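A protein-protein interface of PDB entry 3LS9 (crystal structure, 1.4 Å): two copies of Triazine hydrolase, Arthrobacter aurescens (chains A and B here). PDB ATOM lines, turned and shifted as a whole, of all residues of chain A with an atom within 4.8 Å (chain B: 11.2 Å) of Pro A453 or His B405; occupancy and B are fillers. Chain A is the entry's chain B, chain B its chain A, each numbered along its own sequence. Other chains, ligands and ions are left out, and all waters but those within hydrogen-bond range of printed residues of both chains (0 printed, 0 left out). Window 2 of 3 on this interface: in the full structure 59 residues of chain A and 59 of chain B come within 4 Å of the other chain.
The backbone NH of His B405 sits at hydrogen-bond distance from the backbone carbonyl oxygen of Arg A72 (3.0 Å). O of Val B402 lies within hydrogen-bond range of NH1 of Arg A72, at 2.8 Å. A ring nitrogen (NE2) of His B405 sits at hydrogen-bond distance from the backbone carbonyl oxygen of Ala A70, 2.8 Å away. N of Arg A72 sits at hydrogen-bond distance from O of Gly B403. The backbone NH (N) of Asp B406 lies within hydrogen-bond range of the backbone carbonyl oxygen (O) of Ala A73 (3.0 Å).
O of Gly B403 lies close to NE2 of His B405 (3.4 Å). The guanidinium group (NH1) of Arg B401 lies within hydrogen-bond range of the backbone carbonyl oxygen (O) of Gly B410, at 3.1 Å. N of Ile B409 lies within hydrogen-bond range of OD1 of Asp B406, 3.3 Å away. The backbone carbonyl oxygen (O) of Gly B410 lies within hydrogen-bond range of the side-chain hydroxyl (OG1) of Thr B414, at 2.7 Å. The side-chain carboxylate (OD2) of Asp B406 is in salt-bridge range of the guanidinium group (NH2) of Arg B361 (2.9 Å). The side-chain carboxylate of Asp B406 sits at hydrogen-bond distance from the backbone NH of Ala B408, at 3.0 Å.
Among the printed residues, pairs that only touch across the chains: Ala A70 with Gly B403, Arg A72 with Asp B400, Arg A72 with Val B404, Ala A73 with Val B404, Ala A73 with His B405, Ala A73 with Ile B409, Ala A73 with Gly B410, Ile A74 with His B405, Pro A75 with Asp B406, Pro A75 with Ile B409, Ile A452 with Gly B403, Ile A452 with His B405 and Pro A453 with His B405.
Printed residues of chain B within 4 Å of Pro A453: His B405 (3.2 Å). Of chain A, only Ala A70 (2.8 Å), Arg A72 (3.0 Å), Ala A73 (3.7 Å), Ile A74 (3.6 Å), Ile A452 (3.9 Å) and Pro A453 (3.2 Å) come within 4 Å of His B405. Of chain B, only Gly B403 and His B405 come within 4 Å of Ala A70. Ala A73 touches just these residues of chain B: Val B404 (3.9 Å), His B405 (3.7 Å), Asp B406 (3.0 Å), Ile B409 (3.7 Å) and Gly B410 (3.7 Å). Of chain B, only His B405 (3.6 Å) comes within 4 Å of Ile A74. No residue of chain B comes within 4 Å of Trp A96. Ile A452 touches just these residues of chain B: Gly B403 (3.96 Å) and His B405 (3.9 Å). Printed residues of chain B within 4 Å of Pro A75: Asp B406 and Ile B409. Of the printed residues of chain A, Gly B410 touches Ala A73 (3.7 Å). Printed residues of chain A within 4 Å of Gly B403: Ala A70 (3.9 Å), Arg A72 (3.2 Å) and Ile A452 (3.96 Å). Of the printed residues of chain A, Asp B406 touches Ala A73 and Pro A75. Ile B54 touches none of the printed residues of chain A. Met B413 touches none of the printed residues of chain A. The nearest residue of chain A that does not touch His B405 is Met A71 (4.2 Å). The nearest printed residue of chain B that does not touch Arg A72 is Thr B414 (4.1 Å).
Of the 12 printed residues of chain A, 7 touch a printed residue of chain B. Printed residues of chain A that touch a printed residue of chain B: Ala A70, Arg A72, Ala A73, Ile A74, Pro A75, Ile A452 and Pro A453. Printed residues of chain B that touch a printed residue of chain A: Asp B400, Val B402, Gly B403, Val B404, His B405, Asp B406, Ile B409 and Gly B410. Hydrophobic or aromatic side chains of chain B within 4 Å of the printed part of chain A: Val B404, His B405 and Ile B409. Among the printed residues, no Asp or Glu carboxylate lies within 4 Å of a Lys or Arg side-chain nitrogen of the other chain.
No position is printed for both chains.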
ATOM      1  N   ALA A  70      -9.947 -27.666  18.645  1.00  0.00           N
ATOM      2  CA  ALA A  70     -10.500 -27.564  19.991  1.00  0.00           C
ATOM      3  C   ALA A  70      -9.493 -27.918  21.080  1.00  0.00           C
ATOM      4  O   ALA A  70      -9.824 -27.877  22.270  1.00  0.00           O
ATOM      5  CB  ALA A  70     -11.721 -28.465  20.117  1.00  0.00           C
ATOM      6  N   MET A  71      -8.271 -28.258  20.684  1.00  0.00           N
ATOM      7  CA  MET A  71      -7.280 -28.782  21.616  1.00  0.00           C
ATOM      8  C   MET A  71      -5.979 -28.003  21.599  1.00  0.00           C
ATOM      9  O   MET A  71      -4.907 -28.574  21.768  1.00  0.00           O
ATOM     10  CB  MET A  71      -6.966 -30.229  21.260  1.00  0.00           C
ATOM     11  CG  MET A  71      -8.197 -31.103  21.174  1.00  0.00           C
ATOM     12  SD  MET A  71      -7.772 -32.803  20.768  1.00  0.00           S
ATOM     13  CE  MET A  71      -6.900 -33.252  22.254  1.00  0.00           C
ATOM     14  N   ARG A  72      -6.078 -26.699  21.413  1.00  0.00           N
ATOM     15  CA  ARG A  72      -4.903 -25.847  21.310  1.00  0.00           C
ATOM     16  C   ARG A  72      -4.369 -25.420  22.664  1.00  0.00           C
ATOM     17  O   ARG A  72      -5.132 -25.118  23.583  1.00  0.00           O
ATOM     18  CB  ARG A  72      -5.249 -24.591  20.513  1.00  0.00           C
ATOM     19  CG  ARG A  72      -5.446 -24.839  19.041  1.00  0.00           C
ATOM     20  CD  ARG A  72      -5.984 -23.604  18.360  1.00  0.00           C
ATOM     21  NE  ARG A  72      -5.719 -23.680  16.929  1.00  0.00           N
ATOM     22  CZ  ARG A  72      -6.383 -23.004  15.996  1.00  0.00           C
ATOM     23  NH1 ARG A  72      -7.386 -22.201  16.330  1.00  0.00           N
ATOM     24  NH2 ARG A  72      -6.052 -23.151  14.722  1.00  0.00           N
ATOM     25  N   ALA A  73      -3.044 -25.369  22.767  1.00  0.00           N
ATOM     26  CA  ALA A  73      -2.393 -24.756  23.915  1.00  0.00           C
ATOM     27  C   ALA A  73      -2.899 -25.316  25.246  1.00  0.00           C
ATOM     28  O   ALA A  73      -3.187 -24.578  26.187  1.00  0.00           O
ATOM     29  CB  ALA A  73      -2.546 -23.235  23.857  1.00  0.00           C
ATOM     30  N   ILE A  74      -3.019 -26.635  25.290  1.00  0.00           N
ATOM     31  CA  ILE A  74      -3.325 -27.346  26.522  1.00  0.00           C
ATOM     32  C   ILE A  74      -2.023 -27.546  27.298  1.00  0.00           C
ATOM     33  O   ILE A  74      -1.092 -28.159  26.791  1.00  0.00           O
ATOM     34  CB  ILE A  74      -3.977 -28.705  26.209  1.00  0.00           C
ATOM     35  CG1 ILE A  74      -5.351 -28.502  25.571  1.00  0.00           C
ATOM     36  CG2 ILE A  74      -4.085 -29.564  27.474  1.00  0.00           C
ATOM     37  CD1 ILE A  74      -6.015 -29.795  25.131  1.00  0.00           C
ATOM     38  N   PRO A  75      -1.943 -27.016  28.530  1.00  0.00           N
ATOM     39  CA  PRO A  75      -0.660 -27.080  29.249  1.00  0.00           C
ATOM     40  C   PRO A  75      -0.070 -28.485  29.333  1.00  0.00           C
ATOM     41  O   PRO A  75       1.139 -28.647  29.133  1.00  0.00           O
ATOM     42  CB  PRO A  75      -1.012 -26.547  30.643  1.00  0.00           C
ATOM     43  CG  PRO A  75      -2.144 -25.599  30.379  1.00  0.00           C
ATOM     44  CD  PRO A  75      -2.944 -26.209  29.252  1.00  0.00           C
ATOM     45  N   TRP A  96     -14.595 -36.149  26.106  1.00  0.00           N
ATOM     46  CA  TRP A  96     -15.503 -35.083  25.722  1.00  0.00           C
ATOM     47  C   TRP A  96     -16.689 -35.640  24.949  1.00  0.00           C
ATOM     48  O   TRP A  96     -17.826 -35.226  25.156  1.00  0.00           O
ATOM     49  CB  TRP A  96     -14.770 -34.067  24.847  1.00  0.00           C
ATOM     50  CG  TRP A  96     -13.740 -33.255  25.557  1.00  0.00           C
ATOM     51  CD1 TRP A  96     -13.628 -33.055  26.897  1.00  0.00           C
ATOM     52  CD2 TRP A  96     -12.679 -32.509  24.947  1.00  0.00           C
ATOM     53  NE1 TRP A  96     -12.556 -32.228  27.166  1.00  0.00           N
ATOM     54  CE2 TRP A  96     -11.958 -31.886  25.982  1.00  0.00           C
ATOM     55  CE3 TRP A  96     -12.272 -32.314  23.624  1.00  0.00           C
ATOM     56  CZ2 TRP A  96     -10.846 -31.074  25.736  1.00  0.00           C
ATOM     57  CZ3 TRP A  96     -11.170 -31.507  23.382  1.00  0.00           C
ATOM     58  CH2 TRP A  96     -10.471 -30.901  24.432  1.00  0.00           C
ATOM     59  N   LYS A 101     -20.071 -33.576  24.514  1.00  0.00           N
ATOM     60  CA  LYS A 101     -19.461 -32.277  24.222  1.00  0.00           C
ATOM     61  C   LYS A 101     -18.682 -32.275  22.921  1.00  0.00           C
ATOM     62  O   LYS A 101     -17.999 -31.289  22.619  1.00  0.00           O
ATOM     63  CB  LYS A 101     -18.482 -31.904  25.334  1.00  0.00           C
ATOM     64  CG  LYS A 101     -19.083 -31.798  26.720  1.00  0.00           C
ATOM     65  CD  LYS A 101     -17.979 -31.629  27.748  1.00  0.00           C
ATOM     66  CE  LYS A 101     -18.529 -31.179  29.078  1.00  0.00           C
ATOM     67  NZ  LYS A 101     -19.070 -29.800  28.973  1.00  0.00           N
ATOM     68  N   PHE A 102     -18.735 -33.351  22.150  1.00  0.00           N
ATOM     69  CA  PHE A 102     -17.830 -33.469  21.007  1.00  0.00           C
ATOM     70  C   PHE A 102     -18.473 -34.220  19.841  1.00  0.00           C
ATOM     71  O   PHE A 102     -17.837 -35.045  19.193  1.00  0.00           O
ATOM     72  CB  PHE A 102     -16.519 -34.134  21.458  1.00  0.00           C
ATOM     73  CG  PHE A 102     -15.267 -33.570  20.796  1.00  0.00           C
ATOM     74  CD1 PHE A 102     -15.026 -32.204  20.777  1.00  0.00           C
ATOM     75  CD2 PHE A 102     -14.325 -34.417  20.224  1.00  0.00           C
ATOM     76  CE1 PHE A 102     -13.866 -31.685  20.177  1.00  0.00           C
ATOM     77  CE2 PHE A 102     -13.162 -33.899  19.624  1.00  0.00           C
ATOM     78  CZ  PHE A 102     -12.946 -32.531  19.610  1.00  0.00           C
ATOM     79  N   LEU A 451     -18.615 -23.545  22.138  1.00  0.00           N
ATOM     80  CA  LEU A 451     -18.669 -25.001  22.022  1.00  0.00           C
ATOM     81  C   LEU A 451     -17.353 -25.714  22.333  1.00  0.00           C
ATOM     82  O   LEU A 451     -17.296 -26.945  22.312  1.00  0.00           O
ATOM     83  CB  LEU A 451     -19.155 -25.413  20.628  1.00  0.00           C
ATOM     84  CG  LEU A 451     -20.561 -24.993  20.221  1.00  0.00           C
ATOM     85  CD1 LEU A 451     -20.774 -25.258  18.742  1.00  0.00           C
ATOM     86  CD2 LEU A 451     -21.589 -25.741  21.062  1.00  0.00           C
ATOM     87  N   ILE A 452     -16.292 -24.965  22.597  1.00  0.00           N
ATOM     88  CA  ILE A 452     -15.036 -25.611  22.942  1.00  0.00           C
ATOM     89  C   ILE A 452     -15.181 -26.249  24.321  1.00  0.00           C
ATOM     90  O   ILE A 452     -15.539 -25.565  25.280  1.00  0.00           O
ATOM     91  CB  ILE A 452     -13.863 -24.608  22.970  1.00  0.00           C
ATOM     92  CG1 ILE A 452     -13.732 -23.877  21.625  1.00  0.00           C
ATOM     93  CG2 ILE A 452     -12.558 -25.316  23.365  1.00  0.00           C
ATOM     94  CD1 ILE A 452     -13.398 -24.780  20.458  1.00  0.00           C
ATOM     95  N   PRO A 453     -14.910 -27.560  24.424  1.00  0.00           N
ATOM     96  CA  PRO A 453     -14.985 -28.210  25.738  1.00  0.00           C
ATOM     97  C   PRO A 453     -13.948 -27.640  26.702  1.00  0.00           C
ATOM     98  O   PRO A 453     -12.834 -27.282  26.297  1.00  0.00           O
ATOM     99  CB  PRO A 453     -14.652 -29.673  25.426  1.00  0.00           C
ATOM    100  CG  PRO A 453     -14.889 -29.833  23.969  1.00  0.00           C
ATOM    101  CD  PRO A 453     -14.572 -28.511  23.353  1.00  0.00           C
ATOM    102  N   THR B   8      -8.166  -9.863  30.231  1.00  0.00           N
ATOM    103  CA  THR B   8      -8.504 -11.271  30.393  1.00  0.00           C
ATOM    104  C   THR B   8      -7.394 -12.029  31.125  1.00  0.00           C
ATOM    105  O   THR B   8      -7.665 -12.864  31.984  1.00  0.00           O
ATOM    106  CB  THR B   8      -8.819 -11.909  29.035  1.00  0.00           C
ATOM    107  OG1 THR B   8     -10.017 -11.319  28.516  1.00  0.00           O
ATOM    108  CG2 THR B   8      -9.000 -13.415  29.152  1.00  0.00           C
ATOM    109  N   ARG B   9      -6.141 -11.726  30.802  1.00  0.00           N
ATOM    110  CA  ARG B   9      -5.016 -12.359  31.461  1.00  0.00           C
ATOM    111  C   ARG B   9      -3.915 -11.329  31.594  1.00  0.00           C
ATOM    112  O   ARG B   9      -3.673 -10.552  30.668  1.00  0.00           O
ATOM    113  CB  ARG B   9      -4.520 -13.552  30.645  1.00  0.00           C
ATOM    114  CG  ARG B   9      -3.383 -14.325  31.291  1.00  0.00           C
ATOM    115  CD  ARG B   9      -3.816 -14.937  32.597  1.00  0.00           C
ATOM    116  NE  ARG B   9      -4.821 -15.970  32.381  1.00  0.00           N
ATOM    117  CZ  ARG B   9      -4.565 -17.273  32.372  1.00  0.00           C
ATOM    118  NH1 ARG B   9      -3.329 -17.710  32.575  1.00  0.00           N
ATOM    119  NH2 ARG B   9      -5.543 -18.142  32.164  1.00  0.00           N
ATOM    120  N   ILE B  11       0.167 -11.302  32.811  1.00  0.00           N
ATOM    121  CA  ILE B  11       1.325 -12.106  33.181  1.00  0.00           C
ATOM    122  C   ILE B  11       2.372 -11.155  33.741  1.00  0.00           C
ATOM    123  O   ILE B  11       2.885 -10.300  33.012  1.00  0.00           O
ATOM    124  CB  ILE B  11       1.938 -12.800  31.956  1.00  0.00           C
ATOM    125  CG1 ILE B  11       0.861 -13.518  31.133  1.00  0.00           C
ATOM    126  CG2 ILE B  11       3.038 -13.774  32.391  1.00  0.00           C
ATOM    127  CD1 ILE B  11       0.167 -14.639  31.861  1.00  0.00           C
ATOM    128  N   GLU B  19       0.127 -14.534  37.893  1.00  0.00           N
ATOM    129  CA  GLU B  19      -0.724 -14.201  36.767  1.00  0.00           C
ATOM    130  C   GLU B  19      -2.087 -13.827  37.335  1.00  0.00           C
ATOM    131  O   GLU B  19      -2.415 -14.193  38.471  1.00  0.00           O
ATOM    132  CB  GLU B  19      -0.818 -15.383  35.798  1.00  0.00           C
ATOM    133  CG  GLU B  19       0.560 -15.904  35.394  1.00  0.00           C
ATOM    134  CD  GLU B  19       0.562 -16.891  34.244  1.00  0.00           C
ATOM    135  OE1 GLU B  19      -0.510 -17.234  33.702  1.00  0.00           O
ATOM    136  OE2 GLU B  19       1.670 -17.332  33.874  1.00  0.00           O
ATOM    137  N   GLU B  21      -6.415 -13.120  36.235  1.00  0.00           N
ATOM    138  CA  GLU B  21      -7.490 -13.157  35.257  1.00  0.00           C
ATOM    139  C   GLU B  21      -8.479 -12.045  35.563  1.00  0.00           C
ATOM    140  O   GLU B  21      -8.769 -11.766  36.727  1.00  0.00           O
ATOM    141  CB  GLU B  21      -8.196 -14.510  35.294  1.00  0.00           C
ATOM    142  CG  GLU B  21      -7.283 -15.681  35.002  1.00  0.00           C
ATOM    143  CD  GLU B  21      -8.033 -16.980  34.764  1.00  0.00           C
ATOM    144  OE1 GLU B  21      -7.371 -17.990  34.439  1.00  0.00           O
ATOM    145  OE2 GLU B  21      -9.278 -16.993  34.904  1.00  0.00           O
ATOM    146  N   ILE B  54      -4.578 -10.233  26.518  1.00  0.00           N
ATOM    147  CA  ILE B  54      -3.530 -10.640  27.449  1.00  0.00           C
ATOM    148  C   ILE B  54      -2.475  -9.530  27.521  1.00  0.00           C
ATOM    149  O   ILE B  54      -2.066  -8.991  26.485  1.00  0.00           O
ATOM    150  CB  ILE B  54      -2.902 -11.993  27.049  1.00  0.00           C
ATOM    151  CG1 ILE B  54      -1.801 -12.385  28.039  1.00  0.00           C
ATOM    152  CG2 ILE B  54      -2.340 -11.941  25.621  1.00  0.00           C
ATOM    153  CD1 ILE B  54      -1.304 -13.813  27.880  1.00  0.00           C
ATOM    154  N   ALA B 360       6.762 -22.123  26.804  1.00  0.00           N
ATOM    155  CA  ALA B 360       6.275 -20.809  26.407  1.00  0.00           C
ATOM    156  C   ALA B 360       6.527 -19.766  27.488  1.00  0.00           C
ATOM    157  O   ALA B 360       6.971 -18.660  27.201  1.00  0.00           O
ATOM    158  CB  ALA B 360       4.794 -20.869  26.061  1.00  0.00           C
ATOM    159  N   ARG B 361       6.261 -20.107  28.743  1.00  0.00           N
ATOM    160  CA  ARG B 361       6.483 -19.149  29.812  1.00  0.00           C
ATOM    161  C   ARG B 361       7.960 -18.827  30.011  1.00  0.00           C
ATOM    162  O   ARG B 361       8.309 -17.681  30.277  1.00  0.00           O
ATOM    163  CB  ARG B 361       5.821 -19.604  31.115  1.00  0.00           C
ATOM    164  CG  ARG B 361       4.329 -19.356  31.099  1.00  0.00           C
ATOM    165  CD  ARG B 361       3.634 -19.962  32.307  1.00  0.00           C
ATOM    166  NE  ARG B 361       2.247 -19.509  32.370  1.00  0.00           N
ATOM    167  CZ  ARG B 361       1.261 -20.031  31.648  1.00  0.00           C
ATOM    168  NH1 ARG B 361       0.033 -19.541  31.766  1.00  0.00           N
ATOM    169  NH2 ARG B 361       1.507 -21.027  30.812  1.00  0.00           N
ATOM    170  N   LEU B 396      -7.068 -11.854  22.298  1.00  0.00           N
ATOM    171  CA  LEU B 396      -7.219 -13.302  22.404  1.00  0.00           C
ATOM    172  C   LEU B 396      -8.456 -13.792  21.677  1.00  0.00           C
ATOM    173  O   LEU B 396      -8.708 -15.000  21.625  1.00  0.00           O
ATOM    174  CB  LEU B 396      -7.364 -13.701  23.869  1.00  0.00           C
ATOM    175  CG  LEU B 396      -6.177 -13.378  24.764  1.00  0.00           C
ATOM    176  CD1 LEU B 396      -6.573 -13.579  26.215  1.00  0.00           C
ATOM    177  CD2 LEU B 396      -4.992 -14.253  24.401  1.00  0.00           C
ATOM    178  N   GLY B 398      -9.521 -13.472  18.421  1.00  0.00           N
ATOM    179  CA  GLY B 398      -9.523 -13.656  16.984  1.00  0.00           C
ATOM    180  C   GLY B 398      -9.856 -15.085  16.589  1.00  0.00           C
ATOM    181  O   GLY B 398      -9.722 -16.024  17.380  1.00  0.00           O
ATOM    182  N   ASP B 400      -8.320 -17.005  14.757  1.00  0.00           N
ATOM    183  CA  ASP B 400      -7.094 -17.805  14.740  1.00  0.00           C
ATOM    184  C   ASP B 400      -6.625 -18.251  16.125  1.00  0.00           C
ATOM    185  O   ASP B 400      -5.638 -18.978  16.251  1.00  0.00           O
ATOM    186  CB  ASP B 400      -5.975 -17.091  13.956  1.00  0.00           C
ATOM    187  CG  ASP B 400      -5.690 -15.692  14.461  1.00  0.00           C
ATOM    188  OD1 ASP B 400      -6.521 -15.086  15.167  1.00  0.00           O
ATOM    189  OD2 ASP B 400      -4.606 -15.176  14.129  1.00  0.00           O
ATOM    190  N   ARG B 401      -7.341 -17.843  17.162  1.00  0.00           N
ATOM    191  CA  ARG B 401      -6.994 -18.290  18.506  1.00  0.00           C
ATOM    192  C   ARG B 401      -8.167 -18.966  19.212  1.00  0.00           C
ATOM    193  O   ARG B 401      -8.129 -19.173  20.427  1.00  0.00           O
ATOM    194  CB  ARG B 401      -6.429 -17.137  19.338  1.00  0.00           C
ATOM    195  CG  ARG B 401      -5.198 -16.461  18.715  1.00  0.00           C
ATOM    196  CD  ARG B 401      -4.508 -15.617  19.757  1.00  0.00           C
ATOM    197  NE  ARG B 401      -3.568 -14.645  19.207  1.00  0.00           N
ATOM    198  CZ  ARG B 401      -2.288 -14.893  18.960  1.00  0.00           C
ATOM    199  NH1 ARG B 401      -1.772 -16.095  19.161  1.00  0.00           N
ATOM    200  NH2 ARG B 401      -1.521 -13.921  18.489  1.00  0.00           N
ATOM    201  N   VAL B 402      -9.189 -19.336  18.453  1.00  0.00           N
ATOM    202  CA  VAL B 402     -10.288 -20.110  19.010  1.00  0.00           C
ATOM    203  C   VAL B 402      -9.744 -21.477  19.413  1.00  0.00           C
ATOM    204  O   VAL B 402      -8.924 -22.064  18.711  1.00  0.00           O
ATOM    205  CB  VAL B 402     -11.422 -20.249  17.976  1.00  0.00           C
ATOM    206  CG1 VAL B 402     -12.434 -21.300  18.401  1.00  0.00           C
ATOM    207  CG2 VAL B 402     -12.121 -18.914  17.784  1.00  0.00           C
ATOM    208  N   GLY B 403     -10.188 -21.983  20.557  1.00  0.00           N
ATOM    209  CA  GLY B 403      -9.764 -23.295  21.004  1.00  0.00           C
ATOM    210  C   GLY B 403      -8.532 -23.283  21.891  1.00  0.00           C
ATOM    211  O   GLY B 403      -8.093 -24.337  22.332  1.00  0.00           O
ATOM    212  N   VAL B 404      -7.965 -22.102  22.129  1.00  0.00           N
ATOM    213  CA  VAL B 404      -6.789 -21.970  22.979  1.00  0.00           C
ATOM    214  C   VAL B 404      -7.178 -22.123  24.447  1.00  0.00           C
ATOM    215  O   VAL B 404      -8.080 -21.442  24.927  1.00  0.00           O
ATOM    216  CB  VAL B 404      -6.103 -20.600  22.754  1.00  0.00           C
ATOM    217  CG1 VAL B 404      -5.124 -20.276  23.880  1.00  0.00           C
ATOM    218  CG2 VAL B 404      -5.381 -20.572  21.399  1.00  0.00           C
ATOM    219  N   HIS B 405      -6.497 -23.010  25.159  1.00  0.00           N
ATOM    220  CA  HIS B 405      -6.843 -23.252  26.559  1.00  0.00           C
ATOM    221  C   HIS B 405      -6.003 -22.426  27.534  1.00  0.00           C
ATOM    222  O   HIS B 405      -6.492 -21.997  28.575  1.00  0.00           O
ATOM    223  CB  HIS B 405      -6.795 -24.746  26.859  1.00  0.00           C
ATOM    224  CG  HIS B 405      -7.841 -25.522  26.121  1.00  0.00           C
ATOM    225  ND1 HIS B 405      -9.053 -25.868  26.685  1.00  0.00           N
ATOM    226  CD2 HIS B 405      -7.877 -25.981  24.849  1.00  0.00           C
ATOM    227  CE1 HIS B 405      -9.777 -26.526  25.797  1.00  0.00           C
ATOM    228  NE2 HIS B 405      -9.088 -26.606  24.672  1.00  0.00           N
ATOM    229  N   ASP B 406      -4.749 -22.178  27.178  1.00  0.00           N
ATOM    230  CA  ASP B 406      -3.850 -21.366  27.994  1.00  0.00           C
ATOM    231  C   ASP B 406      -3.358 -20.212  27.135  1.00  0.00           C
ATOM    232  O   ASP B 406      -2.617 -20.433  26.180  1.00  0.00           O
ATOM    233  CB  ASP B 406      -2.668 -22.226  28.462  1.00  0.00           C
ATOM    234  CG  ASP B 406      -1.676 -21.466  29.328  1.00  0.00           C
ATOM    235  OD1 ASP B 406      -1.463 -20.258  29.094  1.00  0.00           O
ATOM    236  OD2 ASP B 406      -1.069 -22.097  30.224  1.00  0.00           O
ATOM    237  N   PRO B 407      -3.768 -18.979  27.461  1.00  0.00           N
ATOM    238  CA  PRO B 407      -3.476 -17.823  26.600  1.00  0.00           C
ATOM    239  C   PRO B 407      -1.987 -17.526  26.448  1.00  0.00           C
ATOM    240  O   PRO B 407      -1.584 -17.031  25.396  1.00  0.00           O
ATOM    241  CB  PRO B 407      -4.176 -16.656  27.316  1.00  0.00           C
ATOM    242  CG  PRO B 407      -5.157 -17.286  28.245  1.00  0.00           C
ATOM    243  CD  PRO B 407      -4.590 -18.616  28.629  1.00  0.00           C
ATOM    244  N   ALA B 408      -1.180 -17.798  27.463  1.00  0.00           N
ATOM    245  CA  ALA B 408       0.261 -17.544  27.368  1.00  0.00           C
ATOM    246  C   ALA B 408       0.904 -18.508  26.377  1.00  0.00           C
ATOM    247  O   ALA B 408       1.707 -18.105  25.536  1.00  0.00           O
ATOM    248  CB  ALA B 408       0.912 -17.669  28.737  1.00  0.00           C
ATOM    249  N   ILE B 409       0.552 -19.787  26.463  1.00  0.00           N
ATOM    250  CA  ILE B 409       1.033 -20.749  25.486  1.00  0.00           C
ATOM    251  C   ILE B 409       0.502 -20.380  24.096  1.00  0.00           C
ATOM    252  O   ILE B 409       1.231 -20.439  23.100  1.00  0.00           O
ATOM    253  CB  ILE B 409       0.625 -22.192  25.867  1.00  0.00           C
ATOM    254  CG1 ILE B 409       1.306 -22.581  27.183  1.00  0.00           C
ATOM    255  CG2 ILE B 409       1.015 -23.155  24.777  1.00  0.00           C
ATOM    256  CD1 ILE B 409       0.801 -23.889  27.779  1.00  0.00           C
ATOM    257  N   GLY B 410      -0.758 -19.961  24.033  1.00  0.00           N
ATOM    258  CA  GLY B 410      -1.366 -19.577  22.770  1.00  0.00           C
ATOM    259  C   GLY B 410      -0.615 -18.453  22.068  1.00  0.00           C
ATOM    260  O   GLY B 410      -0.563 -18.421  20.841  1.00  0.00           O
ATOM    261  N   LEU B 411      -0.016 -17.542  22.832  1.00  0.00           N
ATOM    262  CA  LEU B 411       0.732 -16.434  22.229  1.00  0.00           C
ATOM    263  C   LEU B 411       1.906 -16.928  21.394  1.00  0.00           C
ATOM    264  O   LEU B 411       2.294 -16.305  20.397  1.00  0.00           O
ATOM    265  CB  LEU B 411       1.265 -15.516  23.321  1.00  0.00           C
ATOM    266  CG  LEU B 411       0.561 -14.204  23.639  1.00  0.00           C
ATOM    267  CD1 LEU B 411       1.472 -13.397  24.545  1.00  0.00           C
ATOM    268  CD2 LEU B 411       0.238 -13.410  22.378  1.00  0.00           C
ATOM    269  N   ILE B 412       2.488 -18.040  21.812  1.00  0.00           N
ATOM    270  CA  ILE B 412       3.636 -18.640  21.141  1.00  0.00           C
ATOM    271  C   ILE B 412       3.246 -19.675  20.087  1.00  0.00           C
ATOM    272  O   ILE B 412       3.936 -19.850  19.076  1.00  0.00           O
ATOM    273  CB  ILE B 412       4.547 -19.365  22.168  1.00  0.00           C
ATOM    274  CG1 ILE B 412       4.944 -18.415  23.296  1.00  0.00           C
ATOM    275  CG2 ILE B 412       5.769 -19.962  21.480  1.00  0.00           C
ATOM    276  CD1 ILE B 412       5.635 -17.175  22.805  1.00  0.00           C
ATOM    277  N   MET B 413       2.144 -20.370  20.325  1.00  0.00           N
ATOM    278  CA  MET B 413       1.844 -21.569  19.552  1.00  0.00           C
ATOM    279  C   MET B 413       0.732 -21.422  18.525  1.00  0.00           C
ATOM    280  O   MET B 413       0.471 -22.361  17.777  1.00  0.00           O
ATOM    281  CB  MET B 413       1.530 -22.744  20.488  1.00  0.00           C
ATOM    282  CG  MET B 413       2.684 -23.100  21.417  1.00  0.00           C
ATOM    283  SD  MET B 413       4.095 -23.808  20.552  1.00  0.00           S
ATOM    284  CE  MET B 413       3.474 -25.426  20.107  1.00  0.00           C
ATOM    285  N   THR B 414       0.067 -20.269  18.498  1.00  0.00           N
ATOM    286  CA  THR B 414      -1.052 -20.084  17.571  1.00  0.00           C
ATOM    287  C   THR B 414      -0.973 -18.720  16.920  1.00  0.00           C
ATOM    288  O   THR B 414      -0.191 -17.864  17.343  1.00  0.00           O
ATOM    289  CB  THR B 414      -2.425 -20.187  18.288  1.00  0.00           C
ATOM    290  OG1 THR B 414      -2.610 -19.061  19.156  1.00  0.00           O
ATOM    291  CG2 THR B 414      -2.534 -21.479  19.078  1.00  0.00           C
